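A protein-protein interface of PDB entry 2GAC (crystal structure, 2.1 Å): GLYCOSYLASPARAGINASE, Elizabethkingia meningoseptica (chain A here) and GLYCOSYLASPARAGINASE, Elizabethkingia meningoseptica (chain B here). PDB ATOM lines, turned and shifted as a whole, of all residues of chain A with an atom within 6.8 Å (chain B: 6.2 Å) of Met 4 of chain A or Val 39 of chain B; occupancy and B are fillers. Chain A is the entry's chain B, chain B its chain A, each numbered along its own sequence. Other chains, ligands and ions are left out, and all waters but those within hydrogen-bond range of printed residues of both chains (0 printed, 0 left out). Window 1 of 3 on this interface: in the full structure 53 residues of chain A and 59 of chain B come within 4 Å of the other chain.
Thr 10 of chain B touches Ile 2 of chain A (OG1 to CA, 3.3 Å). Val 42 of chain B touches Ile 2 of chain A. Ile 2 of chain A touches Val 51 of chain B (N to CG2, 3.9 Å). Met 4 of chain A touches Val 7 of chain B (CG to CG1, 3.6 Å). SD of Met 4 of chain A touches CB of Ala 21 of chain B, at 3.8 Å. Met 4 of chain A touches Gly 38 of chain B. CG1 of Val 7 of chain B touches CB of Ala 6 of chain A, 3.8 Å away. Ala 16 of chain A touches Val 39 of chain B. Ile 89 of chain B touches Ala 16 of chain A. Ile 107 of chain A touches Leu 8 of chain B (CD1 to CB, 3.9 Å).
The backbone carbonyl oxygen (O) of Leu 8 of chain B is in hydrogen-bond range of the backbone NH (N) of Ile 5 of chain A (2.9 Å). The side-chain hydroxyl (OG1) of Thr 10 of chain B is in hydrogen-bond range of the backbone NH (N) of Gly 3 of chain A (2.9 Å). The side-chain carboxylate (OE2) of Glu 43 of chain B sits at hydrogen-bond distance from the side-chain hydroxyl (OG1) of Thr 18 of chain A (2.9 Å).
Of the 14 printed residues of chain A, 11 touch a printed residue of chain B. Hydrophobic or aromatic side chains of chain A within 4 Å of the printed part of chain B: Ile 2, Met 4, Ile 5, Ala 6, Ala 16 and Ile 107. Of the 21 printed residues of chain B, 14 touch a printed residue of chain A. Among the printed residues, 32 pairs touch across the chains. Among the printed residues, no Asp or Glu carboxylate lies within 4 Å of a Lys or Arg side-chain nitrogen of the other chain.
The side-chain amide oxygen (OD1) of Asn 18 of chain B lies within hydrogen-bond range of the side-chain hydroxyl (OG) of Ser 9 of chain B, at 2.8 Å. The side-chain carboxylate of Glu 43 of chain B is in hydrogen-bond range of the backbone NH of Ile 89 of chain B, 3.1 Å away. N of Ile 2 of chain A lies within hydrogen-bond range of O of Thr 18 of chain A (2.9 Å). N of Ala 16 of chain A lies within hydrogen-bond range of O of Met 4 of chain A, 2.9 Å away. The backbone NH (N) of Ala 6 of chain A lies within hydrogen-bond range of the backbone carbonyl oxygen (O) of Ser 14 of chain A. The backbone carbonyl oxygen (O) of Thr 50 of chain A lies within hydrogen-bond range of the backbone NH (N) of Ile 107 of chain A, 3.1 Å away.
Of chain B, only Val 7 (3.6 Å), Leu 8 (3.2 Å), Ser 9 (3.7 Å), Ala 17 (3.6 Å), Asn 18 (3.4 Å), Ala 21 (3.8 Å), Val 35 (3.7 Å), Gly 38 (3.9 Å) and Val 39 (3.9 Å) come within 4 Å of Met 4 of chain A. Of the printed residues of chain A, Val 39 of chain B touches Ile 2, Met 4, Ala 16 and Thr 18. Printed residues of chain A within 4 Å of Asn 18 of chain B: Met 4. Of the printed residues of chain B, Ile 107 of chain A touches Leu 8 (3.9 Å), Ser 9 (3.8 Å) and Thr 10 (3.9 Å). Leu 41 of chain B touches none of the printed residues of chain A. Glu 36 of chain B touches none of the printed residues of chain A. The nearest printed residue of chain A that does not touch Val 39 of chain B is Cys 17 of chain A (5.0 Å). The nearest printed residue of chain A that does not touch Gly 38 of chain B is Ile 2 of chain A (5.2 Å).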
ATOM      1  N   ILE A   2      13.837  15.639  -4.262  1.00  0.00           N
ATOM      2  CA  ILE A   2      12.562  15.840  -3.596  1.00  0.00           C
ATOM      3  C   ILE A   2      12.922  16.635  -2.339  1.00  0.00           C
ATOM      4  O   ILE A   2      13.934  16.360  -1.685  1.00  0.00           O
ATOM      5  CB  ILE A   2      11.837  14.505  -3.177  1.00  0.00           C
ATOM      6  CG1 ILE A   2      10.480  14.913  -2.578  1.00  0.00           C
ATOM      7  CG2 ILE A   2      12.670  13.643  -2.232  1.00  0.00           C
ATOM      8  CD1 ILE A   2       9.594  13.783  -2.011  1.00  0.00           C
ATOM      9  N   GLY A   3      12.171  17.687  -2.057  1.00  0.00           N
ATOM     10  CA  GLY A   3      12.336  18.432  -0.837  1.00  0.00           C
ATOM     11  C   GLY A   3      11.051  18.291  -0.044  1.00  0.00           C
ATOM     12  O   GLY A   3       9.971  18.269  -0.648  1.00  0.00           O
ATOM     13  N   MET A   4      11.130  18.185   1.281  1.00  0.00           N
ATOM     14  CA  MET A   4       9.976  18.009   2.129  1.00  0.00           C
ATOM     15  C   MET A   4      10.205  18.785   3.406  1.00  0.00           C
ATOM     16  O   MET A   4      11.278  18.673   4.013  1.00  0.00           O
ATOM     17  CB  MET A   4       9.790  16.537   2.502  1.00  0.00           C
ATOM     18  CG  MET A   4       8.583  16.274   3.389  1.00  0.00           C
ATOM     19  SD  MET A   4       8.351  14.516   3.734  1.00  0.00           S
ATOM     20  CE  MET A   4       7.427  14.130   2.274  1.00  0.00           C
ATOM     21  N   ILE A   5       9.212  19.557   3.829  1.00  0.00           N
ATOM     22  CA  ILE A   5       9.284  20.332   5.057  1.00  0.00           C
ATOM     23  C   ILE A   5       8.000  20.074   5.852  1.00  0.00           C
ATOM     24  O   ILE A   5       6.928  19.901   5.249  1.00  0.00           O
ATOM     25  CB  ILE A   5       9.453  21.852   4.726  1.00  0.00           C
ATOM     26  CG1 ILE A   5       8.401  22.333   3.723  1.00  0.00           C
ATOM     27  CG2 ILE A   5      10.882  22.059   4.214  1.00  0.00           C
ATOM     28  CD1 ILE A   5       8.446  23.842   3.436  1.00  0.00           C
ATOM     29  N   ALA A   6       8.043  20.016   7.179  1.00  0.00           N
ATOM     30  CA  ALA A   6       6.860  19.700   7.962  1.00  0.00           C
ATOM     31  C   ALA A   6       6.828  20.454   9.275  1.00  0.00           C
ATOM     32  O   ALA A   6       7.891  20.839   9.791  1.00  0.00           O
ATOM     33  CB  ALA A   6       6.830  18.207   8.283  1.00  0.00           C
ATOM     34  N   SER A  14      10.950  20.838  10.552  1.00  0.00           N
ATOM     35  CA  SER A  14      12.137  20.136  10.094  1.00  0.00           C
ATOM     36  C   SER A  14      11.957  19.943   8.592  1.00  0.00           C
ATOM     37  O   SER A  14      10.847  20.118   8.059  1.00  0.00           O
ATOM     38  CB  SER A  14      12.305  18.765  10.757  1.00  0.00           C
ATOM     39  OG  SER A  14      12.672  18.817  12.137  1.00  0.00           O
ATOM     40  N   GLY A  15      13.043  19.622   7.906  1.00  0.00           N
ATOM     41  CA  GLY A  15      13.020  19.454   6.470  1.00  0.00           C
ATOM     42  C   GLY A  15      14.107  18.504   6.005  1.00  0.00           C
ATOM     43  O   GLY A  15      15.100  18.269   6.709  1.00  0.00           O
ATOM     44  N   ALA A  16      13.936  17.976   4.803  1.00  0.00           N
ATOM     45  CA  ALA A  16      14.848  17.010   4.227  1.00  0.00           C
ATOM     46  C   ALA A  16      14.876  17.270   2.730  1.00  0.00           C
ATOM     47  O   ALA A  16      13.883  17.745   2.168  1.00  0.00           O
ATOM     48  CB  ALA A  16      14.345  15.599   4.471  1.00  0.00           C
ATOM     49  N   CYS A  17      15.984  16.998   2.062  1.00  0.00           N
ATOM     50  CA  CYS A  17      16.079  17.265   0.641  1.00  0.00           C
ATOM     51  C   CYS A  17      17.048  16.226   0.112  1.00  0.00           C
ATOM     52  O   CYS A  17      18.099  16.040   0.735  1.00  0.00           O
ATOM     53  CB  CYS A  17      16.600  18.687   0.476  1.00  0.00           C
ATOM     54  SG  CYS A  17      16.500  19.282  -1.221  1.00  0.00           S
ATOM     55  N   THR A  18      16.752  15.481  -0.964  1.00  0.00           N
ATOM     56  CA  THR A  18      17.635  14.441  -1.465  1.00  0.00           C
ATOM     57  C   THR A  18      17.465  14.289  -2.979  1.00  0.00           C
ATOM     58  O   THR A  18      16.380  14.519  -3.547  1.00  0.00           O
ATOM     59  CB  THR A  18      17.322  13.137  -0.668  1.00  0.00           C
ATOM     60  OG1 THR A  18      18.145  12.117  -1.206  1.00  0.00           O
ATOM     61  CG2 THR A  18      15.851  12.742  -0.691  1.00  0.00           C
ATOM     62  N   LEU A  40      17.619  23.756   1.198  1.00  0.00           N
ATOM     63  CA  LEU A  40      16.767  23.619   2.372  1.00  0.00           C
ATOM     64  C   LEU A  40      17.164  24.598   3.461  1.00  0.00           C
ATOM     65  O   LEU A  40      18.362  24.808   3.621  1.00  0.00           O
ATOM     66  CB  LEU A  40      16.899  22.209   2.925  1.00  0.00           C
ATOM     67  CG  LEU A  40      16.276  21.848   4.270  1.00  0.00           C
ATOM     68  CD1 LEU A  40      14.755  21.885   4.196  1.00  0.00           C
ATOM     69  CD2 LEU A  40      16.782  20.477   4.649  1.00  0.00           C
ATOM     70  N   VAL A  42      15.603  25.823   7.556  1.00  0.00           N
ATOM     71  CA  VAL A  42      14.567  25.717   8.581  1.00  0.00           C
ATOM     72  C   VAL A  42      14.924  26.613   9.774  1.00  0.00           C
ATOM     73  O   VAL A  42      16.009  26.449  10.340  1.00  0.00           O
ATOM     74  CB  VAL A  42      14.430  24.255   9.128  1.00  0.00           C
ATOM     75  CG1 VAL A  42      13.249  24.212  10.082  1.00  0.00           C
ATOM     76  CG2 VAL A  42      14.209  23.240   8.015  1.00  0.00           C
ATOM     77  N   THR A  50      11.952  24.671   0.952  1.00  0.00           N
ATOM     78  CA  THR A  50      12.805  23.820   0.131  1.00  0.00           C
ATOM     79  C   THR A  50      12.652  24.352  -1.284  1.00  0.00           C
ATOM     80  O   THR A  50      11.596  24.894  -1.652  1.00  0.00           O
ATOM     81  CB  THR A  50      12.443  22.310  -0.005  1.00  0.00           C
ATOM     82  OG1 THR A  50      11.186  22.035   0.609  1.00  0.00           O
ATOM     83  CG2 THR A  50      13.566  21.476   0.576  1.00  0.00           C
ATOM     84  N   ILE A 107       8.752  26.062  -2.061  1.00  0.00           N
ATOM     85  CA  ILE A 107       7.530  25.821  -1.307  1.00  0.00           C
ATOM     86  C   ILE A 107       7.943  26.279   0.095  1.00  0.00           C
ATOM     87  O   ILE A 107       9.121  26.106   0.463  1.00  0.00           O
ATOM     88  CB  ILE A 107       7.120  24.310  -1.288  1.00  0.00           C
ATOM     89  CG1 ILE A 107       8.248  23.418  -0.783  1.00  0.00           C
ATOM     90  CG2 ILE A 107       6.689  23.914  -2.701  1.00  0.00           C
ATOM     91  CD1 ILE A 107       7.905  21.927  -0.650  1.00  0.00           C
ATOM     92  N   VAL B   7       2.601  18.663   6.212  1.00  0.00           N
ATOM     93  CA  VAL B   7       3.769  18.280   5.412  1.00  0.00           C
ATOM     94  C   VAL B   7       3.597  18.862   4.015  1.00  0.00           C
ATOM     95  O   VAL B   7       2.477  18.807   3.481  1.00  0.00           O
ATOM     96  CB  VAL B   7       3.981  16.783   5.019  1.00  0.00           C
ATOM     97  CG1 VAL B   7       5.467  16.519   5.198  1.00  0.00           C
ATOM     98  CG2 VAL B   7       3.043  15.824   5.729  1.00  0.00           C
ATOM     99  N   LEU B   8       4.654  19.377   3.392  1.00  0.00           N
ATOM    100  CA  LEU B   8       4.621  19.752   1.985  1.00  0.00           C
ATOM    101  C   LEU B   8       5.865  19.138   1.369  1.00  0.00           C
ATOM    102  O   LEU B   8       6.932  19.124   2.013  1.00  0.00           O
ATOM    103  CB  LEU B   8       4.774  21.240   1.636  1.00  0.00           C
ATOM    104  CG  LEU B   8       4.387  22.489   2.408  1.00  0.00           C
ATOM    105  CD1 LEU B   8       4.248  23.599   1.380  1.00  0.00           C
ATOM    106  CD2 LEU B   8       3.064  22.365   3.135  1.00  0.00           C
ATOM    107  N   SER B   9       5.789  18.631   0.147  1.00  0.00           N
ATOM    108  CA  SER B   9       6.962  18.152  -0.550  1.00  0.00           C
ATOM    109  C   SER B   9       6.904  18.515  -2.024  1.00  0.00           C
ATOM    110  O   SER B   9       5.849  18.964  -2.510  1.00  0.00           O
ATOM    111  CB  SER B   9       7.122  16.640  -0.397  1.00  0.00           C
ATOM    112  OG  SER B   9       5.962  15.859  -0.612  1.00  0.00           O
ATOM    113  N   THR B  10       8.003  18.370  -2.748  1.00  0.00           N
ATOM    114  CA  THR B  10       8.017  18.765  -4.143  1.00  0.00           C
ATOM    115  C   THR B  10       7.578  17.678  -5.117  1.00  0.00           C
ATOM    116  O   THR B  10       7.854  16.484  -4.931  1.00  0.00           O
ATOM    117  CB  THR B  10       9.448  19.265  -4.489  1.00  0.00           C
ATOM    118  OG1 THR B  10      10.348  18.188  -4.221  1.00  0.00           O
ATOM    119  CG2 THR B  10       9.834  20.524  -3.707  1.00  0.00           C
ATOM    120  N   GLY B  14       5.806  13.513  -4.485  1.00  0.00           N
ATOM    121  CA  GLY B  14       5.592  14.044  -3.164  1.00  0.00           C
ATOM    122  C   GLY B  14       4.243  13.607  -2.581  1.00  0.00           C
ATOM    123  O   GLY B  14       4.187  13.453  -1.366  1.00  0.00           O
ATOM    124  N   ALA B  17       4.958  10.423  -0.956  1.00  0.00           N
ATOM    125  CA  ALA B  17       5.943  10.624   0.114  1.00  0.00           C
ATOM    126  C   ALA B  17       5.250  11.222   1.341  1.00  0.00           C
ATOM    127  O   ALA B  17       5.515  10.863   2.494  1.00  0.00           O
ATOM    128  CB  ALA B  17       7.040  11.590  -0.299  1.00  0.00           C
ATOM    129  N   ASN B  18       4.287  12.118   1.110  1.00  0.00           N
ATOM    130  CA  ASN B  18       3.506  12.752   2.152  1.00  0.00           C
ATOM    131  C   ASN B  18       2.672  11.761   2.940  1.00  0.00           C
ATOM    132  O   ASN B  18       2.511  11.933   4.153  1.00  0.00           O
ATOM    133  CB  ASN B  18       2.568  13.796   1.582  1.00  0.00           C
ATOM    134  CG  ASN B  18       3.168  15.183   1.415  1.00  0.00           C
ATOM    135  OD1 ASN B  18       4.344  15.456   1.629  1.00  0.00           O
ATOM    136  ND2 ASN B  18       2.358  16.141   1.029  1.00  0.00           N
ATOM    137  N   ALA B  21       5.126  10.358   5.429  1.00  0.00           N
ATOM    138  CA  ALA B  21       5.430  11.341   6.465  1.00  0.00           C
ATOM    139  C   ALA B  21       4.255  11.497   7.432  1.00  0.00           C
ATOM    140  O   ALA B  21       4.427  11.642   8.650  1.00  0.00           O
ATOM    141  CB  ALA B  21       5.710  12.703   5.838  1.00  0.00           C
ATOM    142  N   ALA B  34       9.363  12.266  10.512  1.00  0.00           N
ATOM    143  CA  ALA B  34       8.424  12.301   9.404  1.00  0.00           C
ATOM    144  C   ALA B  34       9.050  12.679   8.068  1.00  0.00           C
ATOM    145  O   ALA B  34       8.823  11.970   7.081  1.00  0.00           O
ATOM    146  CB  ALA B  34       7.319  13.287   9.723  1.00  0.00           C
ATOM    147  N   VAL B  35       9.853  13.747   7.972  1.00  0.00           N
ATOM    148  CA  VAL B  35      10.477  14.123   6.707  1.00  0.00           C
ATOM    149  C   VAL B  35      11.537  13.114   6.295  1.00  0.00           C
ATOM    150  O   VAL B  35      11.685  12.862   5.094  1.00  0.00           O
ATOM    151  CB  VAL B  35      11.117  15.548   6.763  1.00  0.00           C
ATOM    152  CG1 VAL B  35       9.983  16.503   7.087  1.00  0.00           C
ATOM    153  CG2 VAL B  35      12.238  15.703   7.784  1.00  0.00           C
ATOM    154  N   GLU B  36      12.274  12.482   7.225  1.00  0.00           N
ATOM    155  CA  GLU B  36      13.226  11.451   6.843  1.00  0.00           C
ATOM    156  C   GLU B  36      12.476  10.277   6.211  1.00  0.00           C
ATOM    157  O   GLU B  36      12.790   9.844   5.096  1.00  0.00           O
ATOM    158  CB  GLU B  36      13.997  10.960   8.061  1.00  0.00           C
ATOM    159  CG  GLU B  36      15.065   9.927   7.692  1.00  0.00           C
ATOM    160  CD  GLU B  36      15.849   9.325   8.844  1.00  0.00           C
ATOM    161  OE1 GLU B  36      15.460   9.436  10.000  1.00  0.00           O
ATOM    162  OE2 GLU B  36      16.872   8.699   8.596  1.00  0.00           O
ATOM    163  N   LYS B  37      11.434   9.787   6.885  1.00  0.00           N
ATOM    164  CA  LYS B  37      10.635   8.701   6.348  1.00  0.00           C
ATOM    165  C   LYS B  37       9.973   9.043   5.018  1.00  0.00           C
ATOM    166  O   LYS B  37      10.004   8.221   4.097  1.00  0.00           O
ATOM    167  CB  LYS B  37       9.578   8.304   7.368  1.00  0.00           C
ATOM    168  CG  LYS B  37      10.304   7.458   8.387  1.00  0.00           C
ATOM    169  CD  LYS B  37       9.399   6.895   9.457  1.00  0.00           C
ATOM    170  CE  LYS B  37      10.218   6.040  10.417  1.00  0.00           C
ATOM    171  NZ  LYS B  37      10.884   4.965   9.710  1.00  0.00           N
ATOM    172  N   GLY B  38       9.440  10.251   4.884  1.00  0.00           N
ATOM    173  CA  GLY B  38       8.836  10.695   3.639  1.00  0.00           C
ATOM    174  C   GLY B  38       9.797  10.626   2.456  1.00  0.00           C
ATOM    175  O   GLY B  38       9.518   9.937   1.466  1.00  0.00           O
ATOM    176  N   VAL B  39      10.965  11.269   2.519  1.00  0.00           N
ATOM    177  CA  VAL B  39      11.859  11.262   1.360  1.00  0.00           C
ATOM    178  C   VAL B  39      12.515   9.911   1.117  1.00  0.00           C
ATOM    179  O   VAL B  39      12.754   9.558  -0.047  1.00  0.00           O
ATOM    180  CB  VAL B  39      12.957  12.364   1.494  1.00  0.00           C
ATOM    181  CG1 VAL B  39      12.251  13.708   1.596  1.00  0.00           C
ATOM    182  CG2 VAL B  39      13.879  12.135   2.673  1.00  0.00           C
ATOM    183  N   ARG B  40      12.739   9.097   2.165  1.00  0.00           N
ATOM    184  CA  ARG B  40      13.306   7.763   1.999  1.00  0.00           C
ATOM    185  C   ARG B  40      12.461   6.883   1.087  1.00  0.00           C
ATOM    186  O   ARG B  40      12.987   6.065   0.350  1.00  0.00           O
ATOM    187  CB  ARG B  40      13.409   7.012   3.304  1.00  0.00           C
ATOM    188  CG  ARG B  40      14.516   7.316   4.263  1.00  0.00           C
ATOM    189  CD  ARG B  40      14.322   6.210   5.271  1.00  0.00           C
ATOM    190  NE  ARG B  40      15.629   5.858   5.756  1.00  0.00           N
ATOM    191  CZ  ARG B  40      16.216   4.681   5.555  1.00  0.00           C
ATOM    192  NH1 ARG B  40      15.642   3.673   4.886  1.00  0.00           N
ATOM    193  NH2 ARG B  40      17.486   4.607   5.943  1.00  0.00           N
ATOM    194  N   LEU B  41      11.134   7.059   1.069  1.00  0.00           N
ATOM    195  CA  LEU B  41      10.253   6.312   0.180  1.00  0.00           C
ATOM    196  C   LEU B  41      10.658   6.499  -1.283  1.00  0.00           C
ATOM    197  O   LEU B  41      10.728   5.554  -2.070  1.00  0.00           O
ATOM    198  CB  LEU B  41       8.817   6.789   0.378  1.00  0.00           C
ATOM    199  CG  LEU B  41       7.727   6.187  -0.500  1.00  0.00           C
ATOM    200  CD1 LEU B  41       7.521   4.729  -0.134  1.00  0.00           C
ATOM    201  CD2 LEU B  41       6.434   6.925  -0.287  1.00  0.00           C
ATOM    202  N   VAL B  42      10.997   7.736  -1.642  1.00  0.00           N
ATOM    203  CA  VAL B  42      11.350   8.085  -3.005  1.00  0.00           C
ATOM    204  C   VAL B  42      12.767   7.605  -3.277  1.00  0.00           C
ATOM    205  O   VAL B  42      13.008   7.059  -4.346  1.00  0.00           O
ATOM    206  CB  VAL B  42      11.144   9.614  -3.121  1.00  0.00           C
ATOM    207  CG1 VAL B  42      11.437  10.140  -4.512  1.00  0.00           C
ATOM    208  CG2 VAL B  42       9.665   9.904  -2.871  1.00  0.00           C
ATOM    209  N   GLU B  43      13.724   7.718  -2.339  1.00  0.00           N
ATOM    210  CA  GLU B  43      15.063   7.155  -2.495  1.00  0.00           C
ATOM    211  C   GLU B  43      15.040   5.640  -2.705  1.00  0.00           C
ATOM    212  O   GLU B  43      15.887   5.074  -3.412  1.00  0.00           O
ATOM    213  CB  GLU B  43      15.925   7.408  -1.264  1.00  0.00           C
ATOM    214  CG  GLU B  43      16.275   8.852  -0.893  1.00  0.00           C
ATOM    215  CD  GLU B  43      16.974   9.025   0.455  1.00  0.00           C
ATOM    216  OE1 GLU B  43      16.928   8.168   1.322  1.00  0.00           O
ATOM    217  OE2 GLU B  43      17.597  10.054   0.693  1.00  0.00           O
ATOM    218  N   ASP B  44      14.103   4.966  -2.038  1.00  0.00           N
ATOM    219  CA  ASP B  44      13.934   3.527  -2.145  1.00  0.00           C
ATOM    220  C   ASP B  44      13.392   3.043  -3.481  1.00  0.00           C
ATOM    221  O   ASP B  44      13.706   1.925  -3.924  1.00  0.00           O
ATOM    222  CB  ASP B  44      12.986   3.011  -1.045  1.00  0.00           C
ATOM    223  CG  ASP B  44      13.576   2.820   0.352  1.00  0.00           C
ATOM    224  OD1 ASP B  44      14.786   2.744   0.517  1.00  0.00           O
ATOM    225  OD2 ASP B  44      12.807   2.695   1.302  1.00  0.00           O
ATOM    226  N   VAL B  51      16.018  10.569  -7.608  1.00  0.00           N
ATOM    227  CA  VAL B  51      16.299  10.445  -6.182  1.00  0.00           C
ATOM    228  C   VAL B  51      16.781   9.006  -5.984  1.00  0.00           C
ATOM    229  O   VAL B  51      16.322   8.083  -6.657  1.00  0.00           O
ATOM    230  CB  VAL B  51      15.014  10.677  -5.296  1.00  0.00           C
ATOM    231  CG1 VAL B  51      15.413  10.763  -3.835  1.00  0.00           C
ATOM    232  CG2 VAL B  51      14.335  12.009  -5.569  1.00  0.00           C
ATOM    233  N   ILE B  89      19.699  10.564   2.888  1.00  0.00           N
ATOM    234  CA  ILE B  89      19.128  11.370   3.955  1.00  0.00           C
ATOM    235  C   ILE B  89      19.411  10.823   5.366  1.00  0.00           C
ATOM    236  O   ILE B  89      19.606  11.593   6.307  1.00  0.00           O
ATOM    237  CB  ILE B  89      17.610  11.499   3.676  1.00  0.00           C
ATOM    238  CG1 ILE B  89      17.025  12.614   4.516  1.00  0.00           C
ATOM    239  CG2 ILE B  89      16.890  10.191   3.971  1.00  0.00           C
ATOM    240  CD1 ILE B  89      17.514  14.011   4.095  1.00  0.00           C
